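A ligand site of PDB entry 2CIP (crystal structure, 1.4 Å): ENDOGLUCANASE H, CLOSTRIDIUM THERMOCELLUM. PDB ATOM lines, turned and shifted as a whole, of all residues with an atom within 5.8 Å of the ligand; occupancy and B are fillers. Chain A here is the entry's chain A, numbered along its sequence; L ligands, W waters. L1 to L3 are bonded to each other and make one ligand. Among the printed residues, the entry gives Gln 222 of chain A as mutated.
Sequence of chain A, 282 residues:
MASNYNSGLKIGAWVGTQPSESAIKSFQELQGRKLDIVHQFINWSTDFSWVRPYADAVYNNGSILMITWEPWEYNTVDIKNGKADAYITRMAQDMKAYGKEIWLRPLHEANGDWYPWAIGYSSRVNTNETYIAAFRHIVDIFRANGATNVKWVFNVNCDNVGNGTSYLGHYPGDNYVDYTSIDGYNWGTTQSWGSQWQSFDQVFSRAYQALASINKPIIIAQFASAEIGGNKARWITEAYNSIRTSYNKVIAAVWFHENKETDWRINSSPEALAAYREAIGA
The side-chain carboxylate of Glu 258 is in hydrogen-bond range of an oxygen (O5) of LIG L1 (2.7 Å).
The side-chain amide oxygen (OD1) of Asn 157 sits close to an oxygen (O1) of LG3 L3, 3.1 Å away.
OE2 of Glu 70 sits at hydrogen-bond distance from O1 of LIG L1, 2.6 Å away.
NE2 of Gln 222 is in hydrogen-bond range of O2 of LG2 L2 (2.9 Å).
OE2 of Glu 261 lies within hydrogen-bond range of O4 of LG2 L2 (2.7 Å).
An oxygen (O1) of LIG L1 is in hydrogen-bond range of the side-chain hydroxyl of Tyr 115 (2.7 Å).
The side-chain carboxylate (OE1) of Glu 109 is in hydrogen-bond range of an oxygen (O2) of LG2 L2, 3.1 Å away.
An oxygen (O5) of LIG L1 lies within hydrogen-bond range of the side-chain amino group (NZ) of Lys 260 (2.8 Å).
OH of Tyr 115 lies within hydrogen-bond range of OE2 of Glu 70 (3.5 Å).
The side-chain amide nitrogen of Gln 18 is in hydrogen-bond range of the backbone carbonyl oxygen of Phe 41, 3.0 Å away.
O of Glu 258 sits at hydrogen-bond distance from N of Trp 264 (3.2 Å).
The side-chain carboxylate of Glu 109 lies within hydrogen-bond range of the indole nitrogen of Trp 114, at 2.8 Å.
NE2 of His 108 sits at hydrogen-bond distance from OH of Tyr 115 (3.1 Å).
The side-chain hydroxyl (OH) of Tyr 185 sits at hydrogen-bond distance from the side-chain amide nitrogen (NE2) of Gln 222.
OE1 of Gln 222 lies close to OD2 of Asp 183, at 3.2 Å.
The side-chain carboxylate (OE2) of Glu 109 sits close to the side-chain carboxylate (OD2) of Asp 183 (2.5 Å).
Residues that only touch the ligand: Trp 187, Trp 114, Phe 41, Tyr 185, Phe 256, Trp 14, His 108 and Trp 72.
Of the 23 residues printed, 16 come within 4 Å of the ligand.
The nearest printed residue that does not touch the ligand is Asp 159 (4.2 Å).
Water W2 lies within hydrogen-bond range of the side-chain carboxylate of Asp 159 and an oxygen (O1) of LG3 L3.
Water W4 lies within hydrogen-bond range of N of Tyr 185 (3.0 Å), NE1 of Trp 187 (3.0 Å), O1 of LG3 L3 (3.0 Å) and SG of Cys 158 (3.5 Å).
Water W8 bridges OE2 of Glu 258 (2.7 Å) and O5 of LIG L1 (3.4 Å).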
ATOM      1  N   TRP A  14       1.288   4.379   8.701  1.00  0.00           N
ATOM      2  CA  TRP A  14       1.984   5.063   9.816  1.00  0.00           C
ATOM      3  C   TRP A  14       3.365   5.389   9.231  1.00  0.00           C
ATOM      4  O   TRP A  14       4.037   4.467   8.750  1.00  0.00           O
ATOM      5  CB  TRP A  14       2.104   4.149  11.019  1.00  0.00           C
ATOM      6  CG  TRP A  14       3.199   4.470  12.006  1.00  0.00           C
ATOM      7  CD1 TRP A  14       4.325   3.726  12.188  1.00  0.00           C
ATOM      8  CD2 TRP A  14       3.260   5.575  12.935  1.00  0.00           C
ATOM      9  NE1 TRP A  14       5.097   4.292  13.196  1.00  0.00           N
ATOM     10  CE2 TRP A  14       4.478   5.436  13.653  1.00  0.00           C
ATOM     11  CE3 TRP A  14       2.409   6.654  13.220  1.00  0.00           C
ATOM     12  CZ2 TRP A  14       4.884   6.362  14.645  1.00  0.00           C
ATOM     13  CZ3 TRP A  14       2.816   7.578  14.245  1.00  0.00           C
ATOM     14  CH2 TRP A  14       4.031   7.403  14.933  1.00  0.00           C
ATOM     15  N   GLN A  18       4.976  11.204  14.049  1.00  0.00           N
ATOM     16  CA  GLN A  18       3.659  11.796  13.997  1.00  0.00           C
ATOM     17  C   GLN A  18       3.477  12.550  12.677  1.00  0.00           C
ATOM     18  O   GLN A  18       4.431  13.141  12.154  1.00  0.00           O
ATOM     19  CB  GLN A  18       3.453  12.669  15.241  1.00  0.00           C
ATOM     20  CG  GLN A  18       3.394  11.801  16.567  1.00  0.00           C
ATOM     21  CD  GLN A  18       2.189  10.912  16.690  1.00  0.00           C
ATOM     22  OE1 GLN A  18       1.172  11.107  16.009  1.00  0.00           O
ATOM     23  NE2 GLN A  18       2.264   9.935  17.603  1.00  0.00           N
ATOM     24  N   PHE A  41      -0.689   7.107  16.317  1.00  0.00           N
ATOM     25  CA  PHE A  41      -0.908   6.454  17.616  1.00  0.00           C
ATOM     26  C   PHE A  41      -0.911   7.529  18.680  1.00  0.00           C
ATOM     27  O   PHE A  41      -0.002   8.392  18.702  1.00  0.00           O
ATOM     28  CB  PHE A  41       0.221   5.472  17.937  1.00  0.00           C
ATOM     29  CG  PHE A  41       0.297   4.310  16.999  1.00  0.00           C
ATOM     30  CD1 PHE A  41      -0.295   3.084  17.337  1.00  0.00           C
ATOM     31  CD2 PHE A  41       0.959   4.421  15.770  1.00  0.00           C
ATOM     32  CE1 PHE A  41      -0.241   1.995  16.479  1.00  0.00           C
ATOM     33  CE2 PHE A  41       1.060   3.334  14.897  1.00  0.00           C
ATOM     34  CZ  PHE A  41       0.448   2.109  15.267  1.00  0.00           C
ATOM     35  N   GLU A  70      -4.563   4.337  22.472  1.00  0.00           N
ATOM     36  CA  GLU A  70      -3.983   3.298  23.340  1.00  0.00           C
ATOM     37  C   GLU A  70      -4.127   3.651  24.824  1.00  0.00           C
ATOM     38  O   GLU A  70      -3.465   4.571  25.293  1.00  0.00           O
ATOM     39  CB  GLU A  70      -2.493   3.209  23.067  1.00  0.00           C
ATOM     40  CG  GLU A  70      -2.147   2.773  21.639  1.00  0.00           C
ATOM     41  CD  GLU A  70      -0.674   2.548  21.441  1.00  0.00           C
ATOM     42  OE1 GLU A  70       0.160   3.362  21.938  1.00  0.00           O
ATOM     43  OE2 GLU A  70      -0.338   1.561  20.771  1.00  0.00           O
ATOM     44  N   TRP A  72      -2.869   3.163  27.747  1.00  0.00           N
ATOM     45  CA  TRP A  72      -1.866   2.779  28.725  1.00  0.00           C
ATOM     46  C   TRP A  72      -2.299   3.185  30.113  1.00  0.00           C
ATOM     47  O   TRP A  72      -1.903   2.563  31.136  1.00  0.00           O
ATOM     48  CB  TRP A  72      -0.524   3.416  28.377  1.00  0.00           C
ATOM     49  CG  TRP A  72      -0.014   3.000  27.030  1.00  0.00           C
ATOM     50  CD1 TRP A  72      -0.114   3.713  25.873  1.00  0.00           C
ATOM     51  CD2 TRP A  72       0.718   1.804  26.711  1.00  0.00           C
ATOM     52  NE1 TRP A  72       0.488   3.015  24.838  1.00  0.00           N
ATOM     53  CE2 TRP A  72       1.021   1.859  25.328  1.00  0.00           C
ATOM     54  CE3 TRP A  72       1.138   0.694  27.459  1.00  0.00           C
ATOM     55  CZ2 TRP A  72       1.731   0.832  24.673  1.00  0.00           C
ATOM     56  CZ3 TRP A  72       1.862  -0.323  26.822  1.00  0.00           C
ATOM     57  CH2 TRP A  72       2.151  -0.245  25.427  1.00  0.00           C
ATOM     58  N   HIS A 108      -6.646  -1.695  20.726  1.00  0.00           N
ATOM     59  CA  HIS A 108      -6.316  -2.602  19.642  1.00  0.00           C
ATOM     60  C   HIS A 108      -5.479  -3.789  20.118  1.00  0.00           C
ATOM     61  O   HIS A 108      -4.973  -3.850  21.223  1.00  0.00           O
ATOM     62  CB  HIS A 108      -5.641  -1.831  18.475  1.00  0.00           C
ATOM     63  CG  HIS A 108      -4.184  -1.524  18.666  1.00  0.00           C
ATOM     64  ND1 HIS A 108      -3.686  -0.743  19.699  1.00  0.00           N
ATOM     65  CD2 HIS A 108      -3.114  -1.872  17.909  1.00  0.00           C
ATOM     66  CE1 HIS A 108      -2.369  -0.604  19.541  1.00  0.00           C
ATOM     67  NE2 HIS A 108      -2.004  -1.301  18.469  1.00  0.00           N
ATOM     68  N   GLU A 109      -5.361  -4.766  19.226  1.00  0.00           N
ATOM     69  CA  GLU A 109      -4.566  -5.984  19.474  1.00  0.00           C
ATOM     70  C   GLU A 109      -4.874  -6.635  20.818  1.00  0.00           C
ATOM     71  O   GLU A 109      -3.964  -7.160  21.480  1.00  0.00           O
ATOM     72  CB  GLU A 109      -3.072  -5.729  19.302  1.00  0.00           C
ATOM     73  CG  GLU A 109      -2.694  -5.459  17.827  1.00  0.00           C
ATOM     74  CD  GLU A 109      -1.306  -4.858  17.650  1.00  0.00           C
ATOM     75  OE1 GLU A 109      -0.477  -4.828  18.568  1.00  0.00           O
ATOM     76  OE2 GLU A 109      -0.998  -4.369  16.529  1.00  0.00           O
ATOM     77  N   ASP A 113      -0.852 -10.284  24.062  1.00  0.00           N
ATOM     78  CA  ASP A 113      -0.538 -10.251  25.506  1.00  0.00           C
ATOM     79  C   ASP A 113       0.390  -9.097  25.911  1.00  0.00           C
ATOM     80  O   ASP A 113       0.917  -9.050  27.031  1.00  0.00           O
ATOM     81  CB  ASP A 113       0.042 -11.593  26.009  1.00  0.00           C
ATOM     82  CG  ASP A 113       1.418 -11.877  25.469  1.00  0.00           C
ATOM     83  OD1 ASP A 113       1.956 -11.111  24.620  1.00  0.00           O
ATOM     84  OD2 ASP A 113       2.006 -12.901  25.901  1.00  0.00           O
ATOM     85  N   TRP A 114       0.606  -8.154  25.002  1.00  0.00           N
ATOM     86  CA  TRP A 114       1.625  -7.101  25.198  1.00  0.00           C
ATOM     87  C   TRP A 114       1.081  -5.784  25.678  1.00  0.00           C
ATOM     88  O   TRP A 114       1.841  -4.918  26.123  1.00  0.00           O
ATOM     89  CB  TRP A 114       2.501  -6.846  23.951  1.00  0.00           C
ATOM     90  CG  TRP A 114       1.739  -6.797  22.664  1.00  0.00           C
ATOM     91  CD1 TRP A 114       1.210  -5.692  22.032  1.00  0.00           C
ATOM     92  CD2 TRP A 114       1.463  -7.927  21.825  1.00  0.00           C
ATOM     93  NE1 TRP A 114       0.576  -6.095  20.847  1.00  0.00           N
ATOM     94  CE2 TRP A 114       0.746  -7.441  20.704  1.00  0.00           C
ATOM     95  CE3 TRP A 114       1.753  -9.295  21.916  1.00  0.00           C
ATOM     96  CZ2 TRP A 114       0.285  -8.295  19.685  1.00  0.00           C
ATOM     97  CZ3 TRP A 114       1.312 -10.139  20.894  1.00  0.00           C
ATOM     98  CH2 TRP A 114       0.598  -9.629  19.775  1.00  0.00           C
ATOM     99  N   TYR A 115      -0.228  -5.607  25.592  1.00  0.00           N
ATOM    100  CA  TYR A 115      -0.846  -4.361  26.058  1.00  0.00           C
ATOM    101  C   TYR A 115      -1.617  -4.568  27.345  1.00  0.00           C
ATOM    102  O   TYR A 115      -2.242  -5.600  27.541  1.00  0.00           O
ATOM    103  CB  TYR A 115      -1.818  -3.847  25.003  1.00  0.00           C
ATOM    104  CG  TYR A 115      -1.167  -3.314  23.742  1.00  0.00           C
ATOM    105  CD1 TYR A 115      -0.029  -2.471  23.812  1.00  0.00           C
ATOM    106  CD2 TYR A 115      -1.701  -3.605  22.482  1.00  0.00           C
ATOM    107  CE1 TYR A 115       0.541  -1.936  22.676  1.00  0.00           C
ATOM    108  CE2 TYR A 115      -1.142  -3.088  21.324  1.00  0.00           C
ATOM    109  CZ  TYR A 115      -0.017  -2.284  21.440  1.00  0.00           C
ATOM    110  OH  TYR A 115       0.510  -1.748  20.264  1.00  0.00           O
ATOM    111  N   ASN A 157      -5.018  -8.871  16.356  1.00  0.00           N
ATOM    112  CA  ASN A 157      -3.725  -9.303  15.908  1.00  0.00           C
ATOM    113  C   ASN A 157      -3.892 -10.563  15.041  1.00  0.00           C
ATOM    114  O   ASN A 157      -4.800 -11.386  15.267  1.00  0.00           O
ATOM    115  CB  ASN A 157      -2.840  -9.629  17.115  1.00  0.00           C
ATOM    116  CG  ASN A 157      -1.409  -9.819  16.701  1.00  0.00           C
ATOM    117  OD1 ASN A 157      -0.789 -10.944  16.869  1.00  0.00           O
ATOM    118  ND2 ASN A 157      -0.847  -8.783  16.133  1.00  0.00           N
ATOM    119  N   CYS A 158      -2.974 -10.728  14.082  1.00  0.00           N
ATOM    120  CA  CYS A 158      -3.059 -11.889  13.176  1.00  0.00           C
ATOM    121  C   CYS A 158      -3.028 -13.232  13.925  1.00  0.00           C
ATOM    122  O   CYS A 158      -3.617 -14.201  13.475  1.00  0.00           O
ATOM    123  CB  CYS A 158      -1.910 -11.848  12.156  1.00  0.00           C
ATOM    124  SG  CYS A 158      -0.267 -11.807  12.943  1.00  0.00           S
ATOM    125  N   ASP A 159      -2.338 -13.261  15.075  1.00  0.00           N
ATOM    126  CA  ASP A 159      -2.215 -14.455  15.917  1.00  0.00           C
ATOM    127  C   ASP A 159      -2.745 -14.136  17.278  1.00  0.00           C
ATOM    128  O   ASP A 159      -2.497 -13.041  17.809  1.00  0.00           O
ATOM    129  CB  ASP A 159      -0.738 -14.861  16.091  1.00  0.00           C
ATOM    130  CG  ASP A 159      -0.063 -15.268  14.797  1.00  0.00           C
ATOM    131  OD1 ASP A 159      -0.753 -15.757  13.877  1.00  0.00           O
ATOM    132  OD2 ASP A 159       1.176 -15.091  14.717  1.00  0.00           O
ATOM    133  N   VAL A 161      -2.167 -14.457  21.015  1.00  0.00           N
ATOM    134  CA  VAL A 161      -0.943 -14.633  21.818  1.00  0.00           C
ATOM    135  C   VAL A 161      -1.309 -14.397  23.251  1.00  0.00           C
ATOM    136  O   VAL A 161      -1.838 -13.340  23.598  1.00  0.00           O
ATOM    137  CB  VAL A 161       0.173 -13.643  21.391  1.00  0.00           C
ATOM    138  CG1 VAL A 161       1.463 -13.909  22.168  1.00  0.00           C
ATOM    139  CG2 VAL A 161       0.405 -13.700  19.882  1.00  0.00           C
ATOM    140  N   ASP A 183      -3.813  -6.707  12.275  1.00  0.00           N
ATOM    141  CA  ASP A 183      -2.427  -6.297  12.281  1.00  0.00           C
ATOM    142  C   ASP A 183      -1.534  -7.509  12.195  1.00  0.00           C
ATOM    143  O   ASP A 183      -1.851  -8.554  12.749  1.00  0.00           O
ATOM    144  CB  ASP A 183      -2.095  -5.575  13.599  1.00  0.00           C
ATOM    145  CG  ASP A 183      -2.840  -4.297  13.777  1.00  0.00           C
ATOM    146  OD1 ASP A 183      -3.525  -3.858  12.842  1.00  0.00           O
ATOM    147  OD2 ASP A 183      -2.709  -3.698  14.874  1.00  0.00           O
ATOM    148  N   TYR A 185       2.820  -8.980  11.048  1.00  0.00           N
ATOM    149  CA  TYR A 185       4.119  -8.770  10.413  1.00  0.00           C
ATOM    150  C   TYR A 185       4.727 -10.067   9.919  1.00  0.00           C
ATOM    151  O   TYR A 185       4.533 -11.128  10.542  1.00  0.00           O
ATOM    152  CB  TYR A 185       5.104  -8.171  11.437  1.00  0.00           C
ATOM    153  CG  TYR A 185       4.656  -6.836  11.941  1.00  0.00           C
ATOM    154  CD1 TYR A 185       5.106  -5.667  11.369  1.00  0.00           C
ATOM    155  CD2 TYR A 185       3.722  -6.736  12.977  1.00  0.00           C
ATOM    156  CE1 TYR A 185       4.649  -4.403  11.789  1.00  0.00           C
ATOM    157  CE2 TYR A 185       3.272  -5.478  13.417  1.00  0.00           C
ATOM    158  CZ  TYR A 185       3.750  -4.328  12.806  1.00  0.00           C
ATOM    159  OH  TYR A 185       3.272  -3.118  13.274  1.00  0.00           O
ATOM    160  N   TRP A 187       8.048 -11.347  10.342  1.00  0.00           N
ATOM    161  CA  TRP A 187       9.203 -11.058  11.195  1.00  0.00           C
ATOM    162  C   TRP A 187      10.501 -11.616  10.591  1.00  0.00           C
ATOM    163  O   TRP A 187      11.597 -11.321  11.097  1.00  0.00           O
ATOM    164  CB  TRP A 187       8.977 -11.675  12.592  1.00  0.00           C
ATOM    165  CG  TRP A 187       7.842 -11.044  13.339  1.00  0.00           C
ATOM    166  CD1 TRP A 187       6.536 -11.386  13.256  1.00  0.00           C
ATOM    167  CD2 TRP A 187       7.924  -9.958  14.251  1.00  0.00           C
ATOM    168  NE1 TRP A 187       5.790 -10.569  14.080  1.00  0.00           N
ATOM    169  CE2 TRP A 187       6.611  -9.688  14.702  1.00  0.00           C
ATOM    170  CE3 TRP A 187       8.974  -9.184  14.749  1.00  0.00           C
ATOM    171  CZ2 TRP A 187       6.339  -8.681  15.643  1.00  0.00           C
ATOM    172  CZ3 TRP A 187       8.693  -8.179  15.688  1.00  0.00           C
ATOM    173  CH2 TRP A 187       7.380  -7.935  16.091  1.00  0.00           C
ATOM    174  N   GLN A 222      -2.025  -2.461  10.364  1.00  0.00           N
ATOM    175  CA  GLN A 222      -0.550  -2.395  10.535  1.00  0.00           C
ATOM    176  C   GLN A 222      -0.030  -3.644   9.859  1.00  0.00           C
ATOM    177  O   GLN A 222      -0.418  -4.758  10.241  1.00  0.00           O
ATOM    178  CB  GLN A 222      -0.098  -2.458  12.006  1.00  0.00           C
ATOM    179  CG  GLN A 222      -0.615  -1.361  12.888  1.00  0.00           C
ATOM    180  CD  GLN A 222      -0.242  -1.514  14.381  1.00  0.00           C
ATOM    181  OE1 GLN A 222      -0.971  -1.043  15.255  1.00  0.00           O
ATOM    182  NE2 GLN A 222       0.894  -2.157  14.686  1.00  0.00           N
ATOM    183  N   PHE A 256       3.206  -0.193   8.074  1.00  0.00           N
ATOM    184  CA  PHE A 256       3.845   0.296   9.306  1.00  0.00           C
ATOM    185  C   PHE A 256       5.277   0.684   8.966  1.00  0.00           C
ATOM    186  O   PHE A 256       6.178  -0.178   8.996  1.00  0.00           O
ATOM    187  CB  PHE A 256       3.799  -0.846  10.341  1.00  0.00           C
ATOM    188  CG  PHE A 256       4.212  -0.456  11.737  1.00  0.00           C
ATOM    189  CD1 PHE A 256       3.329   0.119  12.631  1.00  0.00           C
ATOM    190  CD2 PHE A 256       5.513  -0.730  12.158  1.00  0.00           C
ATOM    191  CE1 PHE A 256       3.730   0.419  13.931  1.00  0.00           C
ATOM    192  CE2 PHE A 256       5.897  -0.438  13.486  1.00  0.00           C
ATOM    193  CZ  PHE A 256       5.009   0.148  14.351  1.00  0.00           C
ATOM    194  N   GLU A 258       8.416   2.095   9.869  1.00  0.00           N
ATOM    195  CA  GLU A 258       9.258   2.562  10.950  1.00  0.00           C
ATOM    196  C   GLU A 258      10.413   1.591  11.064  1.00  0.00           C
ATOM    197  O   GLU A 258      10.279   0.396  10.931  1.00  0.00           O
ATOM    198  CB  GLU A 258       8.457   2.627  12.261  1.00  0.00           C
ATOM    199  CG  GLU A 258       9.213   3.468  13.319  1.00  0.00           C
ATOM    200  CD  GLU A 258       8.522   3.526  14.667  1.00  0.00           C
ATOM    201  OE1 GLU A 258       7.290   3.387  14.723  1.00  0.00           O
ATOM    202  OE2 GLU A 258       9.218   3.720  15.696  1.00  0.00           O
ATOM    203  N   LYS A 260      12.286   0.084  13.537  1.00  0.00           N
ATOM    204  CA  LYS A 260      11.988  -0.136  14.948  1.00  0.00           C
ATOM    205  C   LYS A 260      12.538  -1.476  15.368  1.00  0.00           C
ATOM    206  O   LYS A 260      13.781  -1.577  15.462  1.00  0.00           O
ATOM    207  CB  LYS A 260      10.472  -0.027  15.181  1.00  0.00           C
ATOM    208  CG  LYS A 260      10.086   0.214  16.638  1.00  0.00           C
ATOM    209  CD  LYS A 260       8.569   0.410  16.757  1.00  0.00           C
ATOM    210  CE  LYS A 260       8.217   0.517  18.228  1.00  0.00           C
ATOM    211  NZ  LYS A 260       6.750   0.807  18.416  1.00  0.00           N
ATOM    212  N   GLU A 261      11.716  -2.492  15.632  1.00  0.00           N
ATOM    213  CA  GLU A 261      12.206  -3.801  16.082  1.00  0.00           C
ATOM    214  C   GLU A 261      13.140  -4.351  15.027  1.00  0.00           C
ATOM    215  O   GLU A 261      14.173  -4.984  15.345  1.00  0.00           O
ATOM    216  CB  GLU A 261      11.061  -4.777  16.375  1.00  0.00           C
ATOM    217  CG  GLU A 261      10.097  -4.302  17.489  1.00  0.00           C
ATOM    218  CD  GLU A 261       8.996  -3.351  17.031  1.00  0.00           C
ATOM    219  OE1 GLU A 261       8.958  -2.923  15.859  1.00  0.00           O
ATOM    220  OE2 GLU A 261       8.140  -2.961  17.866  1.00  0.00           O
ATOM    221  N   TRP A 264      11.213  -2.168   9.266  1.00  0.00           N
ATOM    222  CA  TRP A 264       9.937  -2.409   8.556  1.00  0.00           C
ATOM    223  C   TRP A 264       9.724  -1.496   7.372  1.00  0.00           C
ATOM    224  O   TRP A 264       8.796  -1.732   6.581  1.00  0.00           O
ATOM    225  CB  TRP A 264       8.772  -2.138   9.520  1.00  0.00           C
ATOM    226  CG  TRP A 264       8.772  -2.941  10.809  1.00  0.00           C
ATOM    227  CD1 TRP A 264       8.806  -2.416  12.080  1.00  0.00           C
ATOM    228  CD2 TRP A 264       8.684  -4.357  10.943  1.00  0.00           C
ATOM    229  NE1 TRP A 264       8.721  -3.431  12.982  1.00  0.00           N
ATOM    230  CE2 TRP A 264       8.660  -4.639  12.329  1.00  0.00           C
ATOM    231  CE3 TRP A 264       8.626  -5.427  10.043  1.00  0.00           C
ATOM    232  CZ2 TRP A 264       8.562  -5.939  12.818  1.00  0.00           C
ATOM    233  CZ3 TRP A 264       8.533  -6.732  10.520  1.00  0.00           C
ATOM    234  CH2 TRP A 264       8.523  -6.982  11.902  1.00  0.00           C
HETATM  235  C1  LIG L   1       2.990   1.080  19.996  1.00  0.00           C
HETATM  236  C2  LIG L   1       2.648   2.563  19.864  1.00  0.00           C
HETATM  237  C3  LIG L   1       3.657   3.262  18.950  1.00  0.00           C
HETATM  238  C4  LIG L   1       3.608   2.534  17.594  1.00  0.00           C
HETATM  239  C5  LIG L   1       4.499   3.206  16.556  1.00  0.00           C
HETATM  240  C6  LIG L   1       3.139   0.395  18.624  1.00  0.00           C
HETATM  241  O1  LIG L   1       2.004   0.404  20.777  1.00  0.00           O
HETATM  242  O2  LIG L   1       2.653   3.206  21.159  1.00  0.00           O
HETATM  243  O3  LIG L   1       3.320   4.610  18.784  1.00  0.00           O
HETATM  244  O4  LIG L   1       3.993   1.164  17.802  1.00  0.00           O
HETATM  245  O5  LIG L   1       5.867   2.998  16.943  1.00  0.00           O
HETATM  246  C1  LG2 L   2       2.448  -2.812  18.217  1.00  0.00           C
HETATM  247  C2  LG2 L   2       3.543  -1.826  17.831  1.00  0.00           C
HETATM  248  C3  LG2 L   2       4.863  -2.575  17.586  1.00  0.00           C
HETATM  249  C4  LG2 L   2       4.642  -3.601  16.468  1.00  0.00           C
HETATM  250  C5  LG2 L   2       5.828  -4.543  16.238  1.00  0.00           C
HETATM  251  C6  LG2 L   2       2.777  -4.254  17.889  1.00  0.00           C
HETATM  252  O1  LG2 L   2       3.513  -4.778  18.981  1.00  0.00           O
HETATM  253  O2  LG2 L   2       1.237  -2.516  17.548  1.00  0.00           O
HETATM  254  O3  LG2 L   2       3.734  -0.885  18.877  1.00  0.00           O
HETATM  255  O4  LG2 L   2       5.885  -1.688  17.171  1.00  0.00           O
HETATM  256  O5  LG2 L   2       3.462  -4.393  16.635  1.00  0.00           O
HETATM  257  O6  LG2 L   2       6.305  -5.140  17.434  1.00  0.00           O
HETATM  258  O1  LG3 L   3       2.232 -11.401  16.480  1.00  0.00           O
HETATM  259  C1  LG3 L   3       2.835 -10.683  17.336  1.00  0.00           C
HETATM  260  O2  LG3 L   3       2.712  -9.304  17.218  1.00  0.00           O
HETATM  261  C2  LG3 L   3       3.306  -8.421  18.091  1.00  0.00           C
HETATM  262  C3  LG3 L   3       3.118  -7.053  17.912  1.00  0.00           C
HETATM  263  C4  LG3 L   3       3.666  -6.125  18.824  1.00  0.00           C
HETATM  264  C5  LG3 L   3       4.412  -6.606  19.883  1.00  0.00           C
HETATM  265  C6  LG3 L   3       4.589  -7.982  20.068  1.00  0.00           C
HETATM  266  C7  LG3 L   3       4.031  -8.902  19.181  1.00  0.00           C
HETATM  267  C8  LG3 L   3       4.191 -10.391  19.315  1.00  0.00           C
HETATM  268  C9  LG3 L   3       4.982 -10.977  20.463  1.00  0.00           C
HETATM  269  C10 LG3 L   3       3.590 -11.227  18.386  1.00  0.00           C
HETATM  270  O   HOH W   1       4.137  -1.055  22.587  1.00  0.00           O
HETATM  271  O   HOH W   2       2.899 -13.993  16.274  1.00  0.00           O
HETATM  272  O   HOH W   3       5.123 -13.693  22.663  1.00  0.00           O
HETATM  273  O   HOH W   4       2.834 -10.409  13.663  1.00  0.00           O
HETATM  274  O   HOH W   5       7.749  -6.860  19.263  1.00  0.00           O
HETATM  275  O   HOH W   6       5.650   6.028  18.450  1.00  0.00           O
HETATM  276  O   HOH W   7       2.426   6.524  20.593  1.00  0.00           O
HETATM  277  O   HOH W   8       8.132   5.437  17.430  1.00  0.00           O
